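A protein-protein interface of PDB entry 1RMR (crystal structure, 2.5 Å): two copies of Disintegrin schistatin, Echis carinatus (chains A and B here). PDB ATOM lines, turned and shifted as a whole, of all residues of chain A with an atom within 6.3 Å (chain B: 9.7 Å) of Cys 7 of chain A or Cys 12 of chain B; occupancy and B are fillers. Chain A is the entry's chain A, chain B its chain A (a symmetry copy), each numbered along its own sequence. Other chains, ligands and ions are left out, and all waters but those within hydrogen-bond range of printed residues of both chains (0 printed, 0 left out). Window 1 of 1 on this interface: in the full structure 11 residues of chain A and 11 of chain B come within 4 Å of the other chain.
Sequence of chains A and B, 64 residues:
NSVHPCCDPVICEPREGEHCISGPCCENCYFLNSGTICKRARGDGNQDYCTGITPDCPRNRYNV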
ATOM      1  N   VAL A   3      14.973  27.472  -3.859  1.00  0.00           N
ATOM      2  CA  VAL A   3      15.938  26.720  -4.661  1.00  0.00           C
ATOM      3  C   VAL A   3      17.376  27.089  -4.305  1.00  0.00           C
ATOM      4  O   VAL A   3      17.656  28.232  -3.939  1.00  0.00           O
ATOM      5  N   HIS A   4      18.246  26.087  -4.230  1.00  0.00           N
ATOM      6  CA  HIS A   4      19.668  26.340  -4.027  1.00  0.00           C
ATOM      7  C   HIS A   4      20.178  26.940  -5.329  1.00  0.00           C
ATOM      8  O   HIS A   4      19.731  26.531  -6.400  1.00  0.00           O
ATOM      9  CB  HIS A   4      20.398  25.027  -3.729  1.00  0.00           C
ATOM     10  CG  HIS A   4      21.783  25.216  -3.196  1.00  0.00           C
ATOM     11  ND1 HIS A   4      22.824  25.678  -3.976  1.00  0.00           N
ATOM     12  CD2 HIS A   4      22.270  25.126  -1.935  1.00  0.00           C
ATOM     13  CE1 HIS A   4      23.889  25.872  -3.217  1.00  0.00           C
ATOM     14  NE2 HIS A   4      23.583  25.537  -1.976  1.00  0.00           N
ATOM     15  N   PRO A   5      20.961  28.012  -5.244  1.00  0.00           N
ATOM     16  CA  PRO A   5      21.439  28.707  -6.449  1.00  0.00           C
ATOM     17  C   PRO A   5      22.330  27.827  -7.344  1.00  0.00           C
ATOM     18  O   PRO A   5      22.655  28.227  -8.446  1.00  0.00           O
ATOM     19  CB  PRO A   5      22.257  29.876  -5.888  1.00  0.00           C
ATOM     20  CG  PRO A   5      22.634  29.458  -4.487  1.00  0.00           C
ATOM     21  CD  PRO A   5      21.592  28.500  -4.004  1.00  0.00           C
ATOM     22  N   CYS A   6      22.758  26.665  -6.870  1.00  0.00           N
ATOM     23  CA  CYS A   6      23.593  25.793  -7.675  1.00  0.00           C
ATOM     24  C   CYS A   6      22.732  24.729  -8.338  1.00  0.00           C
ATOM     25  O   CYS A   6      23.187  24.042  -9.260  1.00  0.00           O
ATOM     26  CB  CYS A   6      24.617  25.097  -6.777  1.00  0.00           C
ATOM     27  SG  CYS A   6      25.860  26.173  -6.047  1.00  0.00           S
ATOM     28  N   CYS A   7      21.551  24.499  -7.761  1.00  0.00           N
ATOM     29  CA  CYS A   7      20.680  23.397  -8.156  1.00  0.00           C
ATOM     30  C   CYS A   7      19.852  23.688  -9.409  1.00  0.00           C
ATOM     31  O   CYS A   7      19.233  24.738  -9.536  1.00  0.00           O
ATOM     32  CB  CYS A   7      19.746  23.031  -7.008  1.00  0.00           C
ATOM     33  SG  CYS A   7      18.669  21.627  -7.370  1.00  0.00           S
ATOM     34  N   ASP A   8      19.736  22.692 -10.273  1.00  0.00           N
ATOM     35  CA  ASP A   8      18.791  22.753 -11.365  1.00  0.00           C
ATOM     36  C   ASP A   8      17.570  21.894 -11.038  1.00  0.00           C
ATOM     37  O   ASP A   8      17.635  20.678 -11.161  1.00  0.00           O
ATOM     38  CB  ASP A   8      19.475  22.264 -12.640  1.00  0.00           C
ATOM     39  CG  ASP A   8      18.507  22.126 -13.811  1.00  0.00           C
ATOM     40  OD1 ASP A   8      17.324  22.512 -13.673  1.00  0.00           O
ATOM     41  OD2 ASP A   8      18.825  21.567 -14.879  1.00  0.00           O
ATOM     42  N   PRO A   9      16.455  22.522 -10.662  1.00  0.00           N
ATOM     43  CA  PRO A   9      15.306  21.809 -10.090  1.00  0.00           C
ATOM     44  C   PRO A   9      14.529  20.924 -11.076  1.00  0.00           C
ATOM     45  O   PRO A   9      13.733  20.116 -10.629  1.00  0.00           O
ATOM     46  CB  PRO A   9      14.413  22.941  -9.581  1.00  0.00           C
ATOM     47  CG  PRO A   9      14.741  24.105 -10.435  1.00  0.00           C
ATOM     48  CD  PRO A   9      16.202  23.970 -10.777  1.00  0.00           C
ATOM     49  N   ILE A  11      16.269  18.916 -13.240  1.00  0.00           N
ATOM     50  CA  ILE A  11      17.063  17.682 -13.143  1.00  0.00           C
ATOM     51  C   ILE A  11      17.425  17.188 -11.752  1.00  0.00           C
ATOM     52  O   ILE A  11      17.670  16.005 -11.570  1.00  0.00           O
ATOM     53  CB  ILE A  11      18.320  17.728 -13.992  1.00  0.00           C
ATOM     54  CG1 ILE A  11      18.066  18.522 -15.279  1.00  0.00           C
ATOM     55  CG2 ILE A  11      18.755  16.301 -14.312  1.00  0.00           C
ATOM     56  CD1 ILE A  11      19.166  18.374 -16.342  1.00  0.00           C
ATOM     57  N   CYS A  12      17.426  18.059 -10.755  1.00  0.00           N
ATOM     58  CA  CYS A  12      17.969  17.712  -9.440  1.00  0.00           C
ATOM     59  C   CYS A  12      19.459  17.371  -9.538  1.00  0.00           C
ATOM     60  O   CYS A  12      19.940  16.384  -8.992  1.00  0.00           O
ATOM     61  CB  CYS A  12      17.161  16.634  -8.742  1.00  0.00           C
ATOM     62  SG  CYS A  12      16.689  17.104  -7.071  1.00  0.00           S
ATOM     63  N   GLU A  13      20.109  18.098 -10.433  1.00  0.00           N
ATOM     64  CA  GLU A  13      21.553  18.111 -10.580  1.00  0.00           C
ATOM     65  C   GLU A  13      22.024  19.569 -10.523  1.00  0.00           C
ATOM     66  O   GLU A  13      21.216  20.480 -10.656  1.00  0.00           O
ATOM     67  CB  GLU A  13      21.872  17.540 -11.965  1.00  0.00           C
ATOM     68  CG  GLU A  13      22.824  16.358 -11.948  1.00  0.00           C
ATOM     69  CD  GLU A  13      22.149  15.065 -12.355  1.00  0.00           C
ATOM     70  OE1 GLU A  13      21.455  15.071 -13.401  1.00  0.00           O
ATOM     71  OE2 GLU A  13      22.360  14.046 -11.656  1.00  0.00           O
ATOM     72  N   PRO A  14      23.327  19.793 -10.396  1.00  0.00           N
ATOM     73  CA  PRO A  14      23.869  21.156 -10.405  1.00  0.00           C
ATOM     74  C   PRO A  14      23.656  21.802 -11.770  1.00  0.00           C
ATOM     75  O   PRO A  14      23.715  21.091 -12.769  1.00  0.00           O
ATOM     76  CB  PRO A  14      25.363  20.933 -10.153  1.00  0.00           C
ATOM     77  CG  PRO A  14      25.446  19.603  -9.481  1.00  0.00           C
ATOM     78  CD  PRO A  14      24.341  18.781 -10.045  1.00  0.00           C
ATOM     79  N   ARG A  15      23.496  23.122 -11.834  1.00  0.00           N
ATOM     80  CA  ARG A  15      23.309  23.785 -13.123  1.00  0.00           C
ATOM     81  C   ARG A  15      24.437  23.377 -14.061  1.00  0.00           C
ATOM     82  O   ARG A  15      25.521  23.015 -13.616  1.00  0.00           O
ATOM     83  CB  ARG A  15      23.276  25.303 -12.949  1.00  0.00           C
ATOM     84  CG  ARG A  15      22.132  25.809 -12.065  1.00  0.00           C
ATOM     85  CD  ARG A  15      22.152  27.328 -11.803  1.00  0.00           C
ATOM     86  NE  ARG A  15      20.837  27.957 -12.010  1.00  0.00           N
ATOM     87  CZ  ARG A  15      20.614  29.261 -12.248  1.00  0.00           C
ATOM     88  NH1 ARG A  15      21.619  30.128 -12.351  1.00  0.00           N
ATOM     89  NH2 ARG A  15      19.366  29.704 -12.406  1.00  0.00           N
ATOM     90  N   CYS A  20      28.950  21.178  -8.196  1.00  0.00           N
ATOM     91  CA  CYS A  20      28.438  20.664  -6.923  1.00  0.00           C
ATOM     92  C   CYS A  20      27.434  21.622  -6.316  1.00  0.00           C
ATOM     93  O   CYS A  20      27.266  22.748  -6.792  1.00  0.00           O
ATOM     94  CB  CYS A  20      29.573  20.426  -5.919  1.00  0.00           C
ATOM     95  SG  CYS A  20      30.769  21.785  -5.816  1.00  0.00           S
ATOM     96  N   ILE A  21      26.855  21.211  -5.197  1.00  0.00           N
ATOM     97  CA  ILE A  21      25.810  21.992  -4.557  1.00  0.00           C
ATOM     98  C   ILE A  21      26.352  22.624  -3.292  1.00  0.00           C
ATOM     99  O   ILE A  21      26.380  23.848  -3.152  1.00  0.00           O
ATOM    100  CB  ILE A  21      24.585  21.102  -4.212  1.00  0.00           C
ATOM    101  CG1 ILE A  21      23.981  20.494  -5.491  1.00  0.00           C
ATOM    102  CG2 ILE A  21      23.528  21.921  -3.473  1.00  0.00           C
ATOM    103  CD1 ILE A  21      23.693  21.525  -6.585  1.00  0.00           C
ATOM    104  N   CYS A  29      29.405  26.509  -6.128  1.00  0.00           N
ATOM    105  CA  CYS A  29      29.046  25.481  -7.093  1.00  0.00           C
ATOM    106  C   CYS A  29      30.230  24.791  -7.746  1.00  0.00           C
ATOM    107  O   CYS A  29      30.033  23.883  -8.563  1.00  0.00           O
ATOM    108  CB  CYS A  29      28.110  26.026  -8.176  1.00  0.00           C
ATOM    109  SG  CYS A  29      26.790  27.104  -7.581  1.00  0.00           S
ATOM    110  N   VAL B   3       9.959  22.539 -11.169  1.00  0.00           N
ATOM    111  CA  VAL B   3      10.615  21.555 -10.307  1.00  0.00           C
ATOM    112  C   VAL B   3      10.159  20.134 -10.625  1.00  0.00           C
ATOM    113  O   VAL B   3       9.012  19.918 -11.024  1.00  0.00           O
ATOM    114  N   HIS B   4      11.099  19.194 -10.632  1.00  0.00           N
ATOM    115  CA  HIS B   4      10.755  17.786 -10.796  1.00  0.00           C
ATOM    116  C   HIS B   4      10.076  17.368  -9.500  1.00  0.00           C
ATOM    117  O   HIS B   4      10.477  17.826  -8.430  1.00  0.00           O
ATOM    118  CB  HIS B   4      12.024  16.958 -11.019  1.00  0.00           C
ATOM    119  CG  HIS B   4      11.758  15.570 -11.510  1.00  0.00           C
ATOM    120  ND1 HIS B   4      11.197  14.593 -10.711  1.00  0.00           N
ATOM    121  CD2 HIS B   4      11.857  15.031 -12.749  1.00  0.00           C
ATOM    122  CE1 HIS B   4      10.955  13.516 -11.439  1.00  0.00           C
ATOM    123  NE2 HIS B   4      11.354  13.752 -12.677  1.00  0.00           N
ATOM    124  N   CYS B   6      10.116  14.834  -7.860  1.00  0.00           N
ATOM    125  CA  CYS B   6      10.900  13.973  -6.995  1.00  0.00           C
ATOM    126  C   CYS B   6      11.998  14.783  -6.323  1.00  0.00           C
ATOM    127  O   CYS B   6      12.619  14.317  -5.360  1.00  0.00           O
ATOM    128  CB  CYS B   6      11.553  12.871  -7.830  1.00  0.00           C
ATOM    129  SG  CYS B   6      10.419  11.677  -8.555  1.00  0.00           S
ATOM    130  N   CYS B   7      12.329  15.923  -6.931  1.00  0.00           N
ATOM    131  CA  CYS B   7      13.474  16.731  -6.527  1.00  0.00           C
ATOM    132  C   CYS B   7      13.199  17.623  -5.315  1.00  0.00           C
ATOM    133  O   CYS B   7      12.190  18.317  -5.249  1.00  0.00           O
ATOM    134  CB  CYS B   7      13.945  17.594  -7.692  1.00  0.00           C
ATOM    135  SG  CYS B   7      15.407  18.585  -7.315  1.00  0.00           S
ATOM    136  N   ASP B   8      14.169  17.702  -4.419  1.00  0.00           N
ATOM    137  CA  ASP B   8      14.136  18.689  -3.363  1.00  0.00           C
ATOM    138  C   ASP B   8      15.089  19.836  -3.701  1.00  0.00           C
ATOM    139  O   ASP B   8      16.293  19.693  -3.530  1.00  0.00           O
ATOM    140  CB  ASP B   8      14.532  18.022  -2.048  1.00  0.00           C
ATOM    141  CG  ASP B   8      14.696  19.021  -0.907  1.00  0.00           C
ATOM    142  OD1 ASP B   8      14.399  20.222  -1.101  1.00  0.00           O
ATOM    143  OD2 ASP B   8      15.194  18.706   0.192  1.00  0.00           O
ATOM    144  N   PRO B   9      14.555  20.976  -4.138  1.00  0.00           N
ATOM    145  CA  PRO B   9      15.365  22.051  -4.723  1.00  0.00           C
ATOM    146  C   PRO B   9      16.267  22.803  -3.732  1.00  0.00           C
ATOM    147  O   PRO B   9      17.143  23.524  -4.177  1.00  0.00           O
ATOM    148  CB  PRO B   9      14.317  23.001  -5.305  1.00  0.00           C
ATOM    149  CG  PRO B   9      13.104  22.785  -4.484  1.00  0.00           C
ATOM    150  CD  PRO B   9      13.124  21.332  -4.086  1.00  0.00           C
ATOM    151  N   VAL B  10      16.065  22.640  -2.429  1.00  0.00           N
ATOM    152  CA  VAL B  10      16.979  23.201  -1.444  1.00  0.00           C
ATOM    153  C   VAL B  10      18.196  22.325  -1.226  1.00  0.00           C
ATOM    154  O   VAL B  10      19.243  22.838  -0.859  1.00  0.00           O
ATOM    155  CB  VAL B  10      16.310  23.511  -0.060  1.00  0.00           C
ATOM    156  CG1 VAL B  10      14.987  24.278  -0.220  1.00  0.00           C
ATOM    157  CG2 VAL B  10      16.095  22.239   0.749  1.00  0.00           C
ATOM    158  N   ILE B  11      18.072  21.012  -1.435  1.00  0.00           N
ATOM    159  CA  ILE B  11      19.251  20.132  -1.459  1.00  0.00           C
ATOM    160  C   ILE B  11      19.767  19.685  -2.817  1.00  0.00           C
ATOM    161  O   ILE B  11      20.935  19.353  -2.946  1.00  0.00           O
ATOM    162  CB  ILE B  11      19.088  18.914  -0.569  1.00  0.00           C
ATOM    163  CG1 ILE B  11      18.269  19.269   0.678  1.00  0.00           C
ATOM    164  CG2 ILE B  11      20.469  18.394  -0.181  1.00  0.00           C
ATOM    165  CD1 ILE B  11      18.303  18.202   1.784  1.00  0.00           C
ATOM    166  N   CYS B  12      18.933  19.707  -3.844  1.00  0.00           N
ATOM    167  CA  CYS B  12      19.287  19.092  -5.126  1.00  0.00           C
ATOM    168  C   CYS B  12      19.520  17.587  -4.964  1.00  0.00           C
ATOM    169  O   CYS B  12      20.489  17.020  -5.456  1.00  0.00           O
ATOM    170  CB  CYS B  12      20.442  19.798  -5.811  1.00  0.00           C
ATOM    171  SG  CYS B  12      20.065  20.238  -7.514  1.00  0.00           S
ATOM    172  N   GLU B  13      18.718  17.022  -4.075  1.00  0.00           N
ATOM    173  CA  GLU B  13      18.600  15.589  -3.878  1.00  0.00           C
ATOM    174  C   GLU B  13      17.115  15.217  -3.973  1.00  0.00           C
ATOM    175  O   GLU B  13      16.259  16.090  -3.902  1.00  0.00           O
ATOM    176  CB  GLU B  13      19.098  15.284  -2.462  1.00  0.00           C
ATOM    177  CG  GLU B  13      20.210  14.254  -2.402  1.00  0.00           C
ATOM    178  CD  GLU B  13      21.532  14.853  -1.970  1.00  0.00           C
ATOM    179  OE1 GLU B  13      21.538  15.585  -0.950  1.00  0.00           O
ATOM    180  OE2 GLU B  13      22.559  14.546  -2.623  1.00  0.00           O
ATOM    181  N   PRO B  14      16.806  13.929  -4.063  1.00  0.00           N
ATOM    182  CA  PRO B  14      15.408  13.482  -4.085  1.00  0.00           C
ATOM    183  C   PRO B  14      14.731  13.790  -2.754  1.00  0.00           C
ATOM    184  O   PRO B  14      15.402  13.719  -1.728  1.00  0.00           O
ATOM    185  CB  PRO B  14      15.535  11.968  -4.277  1.00  0.00           C
ATOM    186  CG  PRO B  14      16.879  11.769  -4.895  1.00  0.00           C
ATOM    187  CD  PRO B  14      17.755  12.835  -4.340  1.00  0.00           C
ATOM    188  N   ARG B  15      13.425  14.042  -2.745  1.00  0.00           N
ATOM    189  CA  ARG B  15      12.732  14.322  -1.489  1.00  0.00           C
ATOM    190  C   ARG B  15      13.027  13.205  -0.498  1.00  0.00           C
ATOM    191  O   ARG B  15      13.328  12.082  -0.891  1.00  0.00           O
ATOM    192  CB  ARG B  15      11.226  14.452  -1.720  1.00  0.00           C
ATOM    193  CG  ARG B  15      10.833  15.594  -2.662  1.00  0.00           C
ATOM    194  CD  ARG B  15       9.326  15.668  -2.979  1.00  0.00           C
ATOM    195  NE  ARG B  15       8.784  17.030  -2.843  1.00  0.00           N
ATOM    196  CZ  ARG B  15       7.490  17.350  -2.661  1.00  0.00           C
ATOM    197  NH1 ARG B  15       6.553  16.412  -2.556  1.00  0.00           N
ATOM    198  NH2 ARG B  15       7.130  18.630  -2.564  1.00  0.00           N
ATOM    199  N   GLU B  16      13.055  13.524   0.789  1.00  0.00           N
ATOM    200  CA  GLU B  16      13.366  12.515   1.798  1.00  0.00           C
ATOM    201  C   GLU B  16      12.379  11.355   1.768  1.00  0.00           C
ATOM    202  O   GLU B  16      11.159  11.556   1.717  1.00  0.00           O
ATOM    203  CB  GLU B  16      13.400  13.120   3.201  1.00  0.00           C
ATOM    204  CG  GLU B  16      14.705  12.856   3.943  1.00  0.00           C
ATOM    205  CD  GLU B  16      14.510  12.047   5.222  1.00  0.00           C
ATOM    206  OE1 GLU B  16      13.550  12.348   5.970  1.00  0.00           O
ATOM    207  OE2 GLU B  16      15.320  11.121   5.491  1.00  0.00           O
ATOM    208  N   CYS B  20      15.109   8.336  -6.116  1.00  0.00           N
ATOM    209  CA  CYS B  20      15.702   8.763  -7.386  1.00  0.00           C
ATOM    210  C   CYS B  20      14.838   9.807  -8.063  1.00  0.00           C
ATOM    211  O   CYS B  20      13.710  10.070  -7.635  1.00  0.00           O
ATOM    212  CB  CYS B  20      15.894   7.578  -8.340  1.00  0.00           C
ATOM    213  SG  CYS B  20      14.460   6.475  -8.451  1.00  0.00           S
ATOM    214  N   ILE B  21      15.327  10.315  -9.185  1.00  0.00           N
ATOM    215  CA  ILE B  21      14.643  11.385  -9.889  1.00  0.00           C
ATOM    216  C   ILE B  21      14.020  10.841 -11.157  1.00  0.00           C
ATOM    217  O   ILE B  21      12.802  10.892 -11.342  1.00  0.00           O
ATOM    218  CB  ILE B  21      15.628  12.533 -10.243  1.00  0.00           C
ATOM    219  CG1 ILE B  21      16.232  13.141  -8.965  1.00  0.00           C
ATOM    220  CG2 ILE B  21      14.911  13.616 -11.049  1.00  0.00           C
ATOM    221  CD1 ILE B  21      15.186  13.540  -7.921  1.00  0.00           C
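The side-chain sulfur (SG) of Cys 7 of chain B is disulfide-bonded to the side-chain sulfur (SG) of Cys 12 of chain A (2.0 Å).
The side-chain sulfur (SG) of Cys 7 of chain A is disulfide-bonded to the side-chain sulfur (SG) of Cys 12 of chain B, at 2.0 Å.
The backbone NH (N) of Glu 13 of chain A lies within hydrogen-bond range of the side-chain sulfur (SG) of Cys 12 of chain B (3.6 Å).
The backbone NH (N) of Glu 13 of chain B sits at hydrogen-bond distance from the side-chain sulfur (SG) of Cys 12 of chain A (3.6 Å).
The backbone NH (N) of His 4 of chain B is in hydrogen-bond range of the backbone carbonyl oxygen (O) of Pro 9 of chain A (2.8 Å).
N of His 4 of chain A sits at hydrogen-bond distance from O of Pro 9 of chain B (2.8 Å).
The backbone NH (N) of Asp 8 of chain A sits at hydrogen-bond distance from the side-chain sulfur (SG) of Cys 12 of chain B (3.7 Å).
The side-chain sulfur of Cys 12 of chain A lies within hydrogen-bond range of the backbone NH of Asp 8 of chain B (3.7 Å).
Among the printed residues, merely in contact across the chains: Pro 9 of chain A with Val 3 of chain B (3.4 Å), Val 3 of chain A with Pro 9 of chain B (3.4 Å), Cys 12 of chain A with Cys 12 of chain B (3.6 Å), Ile 21 of chain A with Cys 12 of chain B (3.6 Å), Cys 12 of chain A with Ile 21 of chain B (3.6 Å), Ile 11 of chain A with Ile 21 of chain B (3.7 Å), Ile 21 of chain A with Ile 11 of chain B (3.7 Å), His 4 of chain A with Val 10 of chain B (3.8 Å), Pro 9 of chain A with Cys 7 of chain B (3.9 Å) and Cys 7 of chain A with Pro 9 of chain B (3.9 Å).
The side-chain sulfur (SG) of Cys 6 of chain A forms a disulfide with the side-chain sulfur (SG) of Cys 29 of chain A.
OD1 of Asp 8 of chain B sits close to N of Val 10 of chain B (3.2 Å).
The backbone carbonyl oxygen (O) of Ile 21 of chain A sits close to a ring nitrogen (NE2) of His 4 of chain A (3.5 Å).
NE2 of His 4 of chain B lies close to O of Ile 21 of chain B, 3.5 Å away.
The backbone NH (N) of Asp 8 of chain B lies within hydrogen-bond range of the backbone carbonyl oxygen (O) of Glu 13 of chain B, at 2.7 Å.
A ring nitrogen (ND1) of His 4 of chain B lies close to the backbone NH (N) of Cys 6 of chain B (3.1 Å).
Cys 7 of chain A touches Cys 12 of chain B, and with the chains exchanged Cys 12 of chain A touches Cys 7 of chain B.
Asp 8 of chain A touches Cys 12 of chain B, and with the chains exchanged Cys 12 of chain A touches Asp 8 of chain B.
Cys 12 of chain A touches its own counterpart, Cys 12 of chain B.
Cys 12 of chain A touches Glu 13 of chain B, and with the chains exchanged Glu 13 of chain A touches Cys 12 of chain B.
Positions printed for both chains: 3, 4, 6, 7, 8, 9, 11, 12, 13, 14, 15, 20 and 21.
Of the printed residues of chain B, His 4 of chain A touches Pro 9 (2.8 Å) and Val 10 (3.8 Å).
Printed residues of chain B within 4 Å of Cys 7 of chain A: Pro 9 (3.9 Å) and Cys 12 (2.0 Å).
Of the printed residues of chain B, Pro 9 of chain A touches Val 3 (3.4 Å), His 4 (2.8 Å) and Cys 7 (3.9 Å).
Cys 12 of chain A touches just these residues of chain B: Cys 7, Asp 8, Cys 12, Glu 13 and Ile 21.
Of chain A, only Cys 7 (2.0 Å), Asp 8 (3.7 Å), Cys 12 (3.6 Å), Glu 13 (3.4 Å) and Ile 21 (3.6 Å) come within 4 Å of Cys 12 of chain B.
Of the printed residues of chain A, Ile 21 of chain B touches Ile 11 (3.7 Å) and Cys 12 (3.6 Å).
Hydrophobic or aromatic side chains of chain A that line the printed part of chain B: His 4 and Ile 21.
Of the 15 printed residues of chain B, 10 touch a printed residue of chain A.
Hydrophobic or aromatic side chains of chain B that line the printed part of chain A: His 4 and Ile 21.
Among the printed residues, no Asp or Glu carboxylate lies within 4 Å of a Lys or Arg side-chain nitrogen of the other chain.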
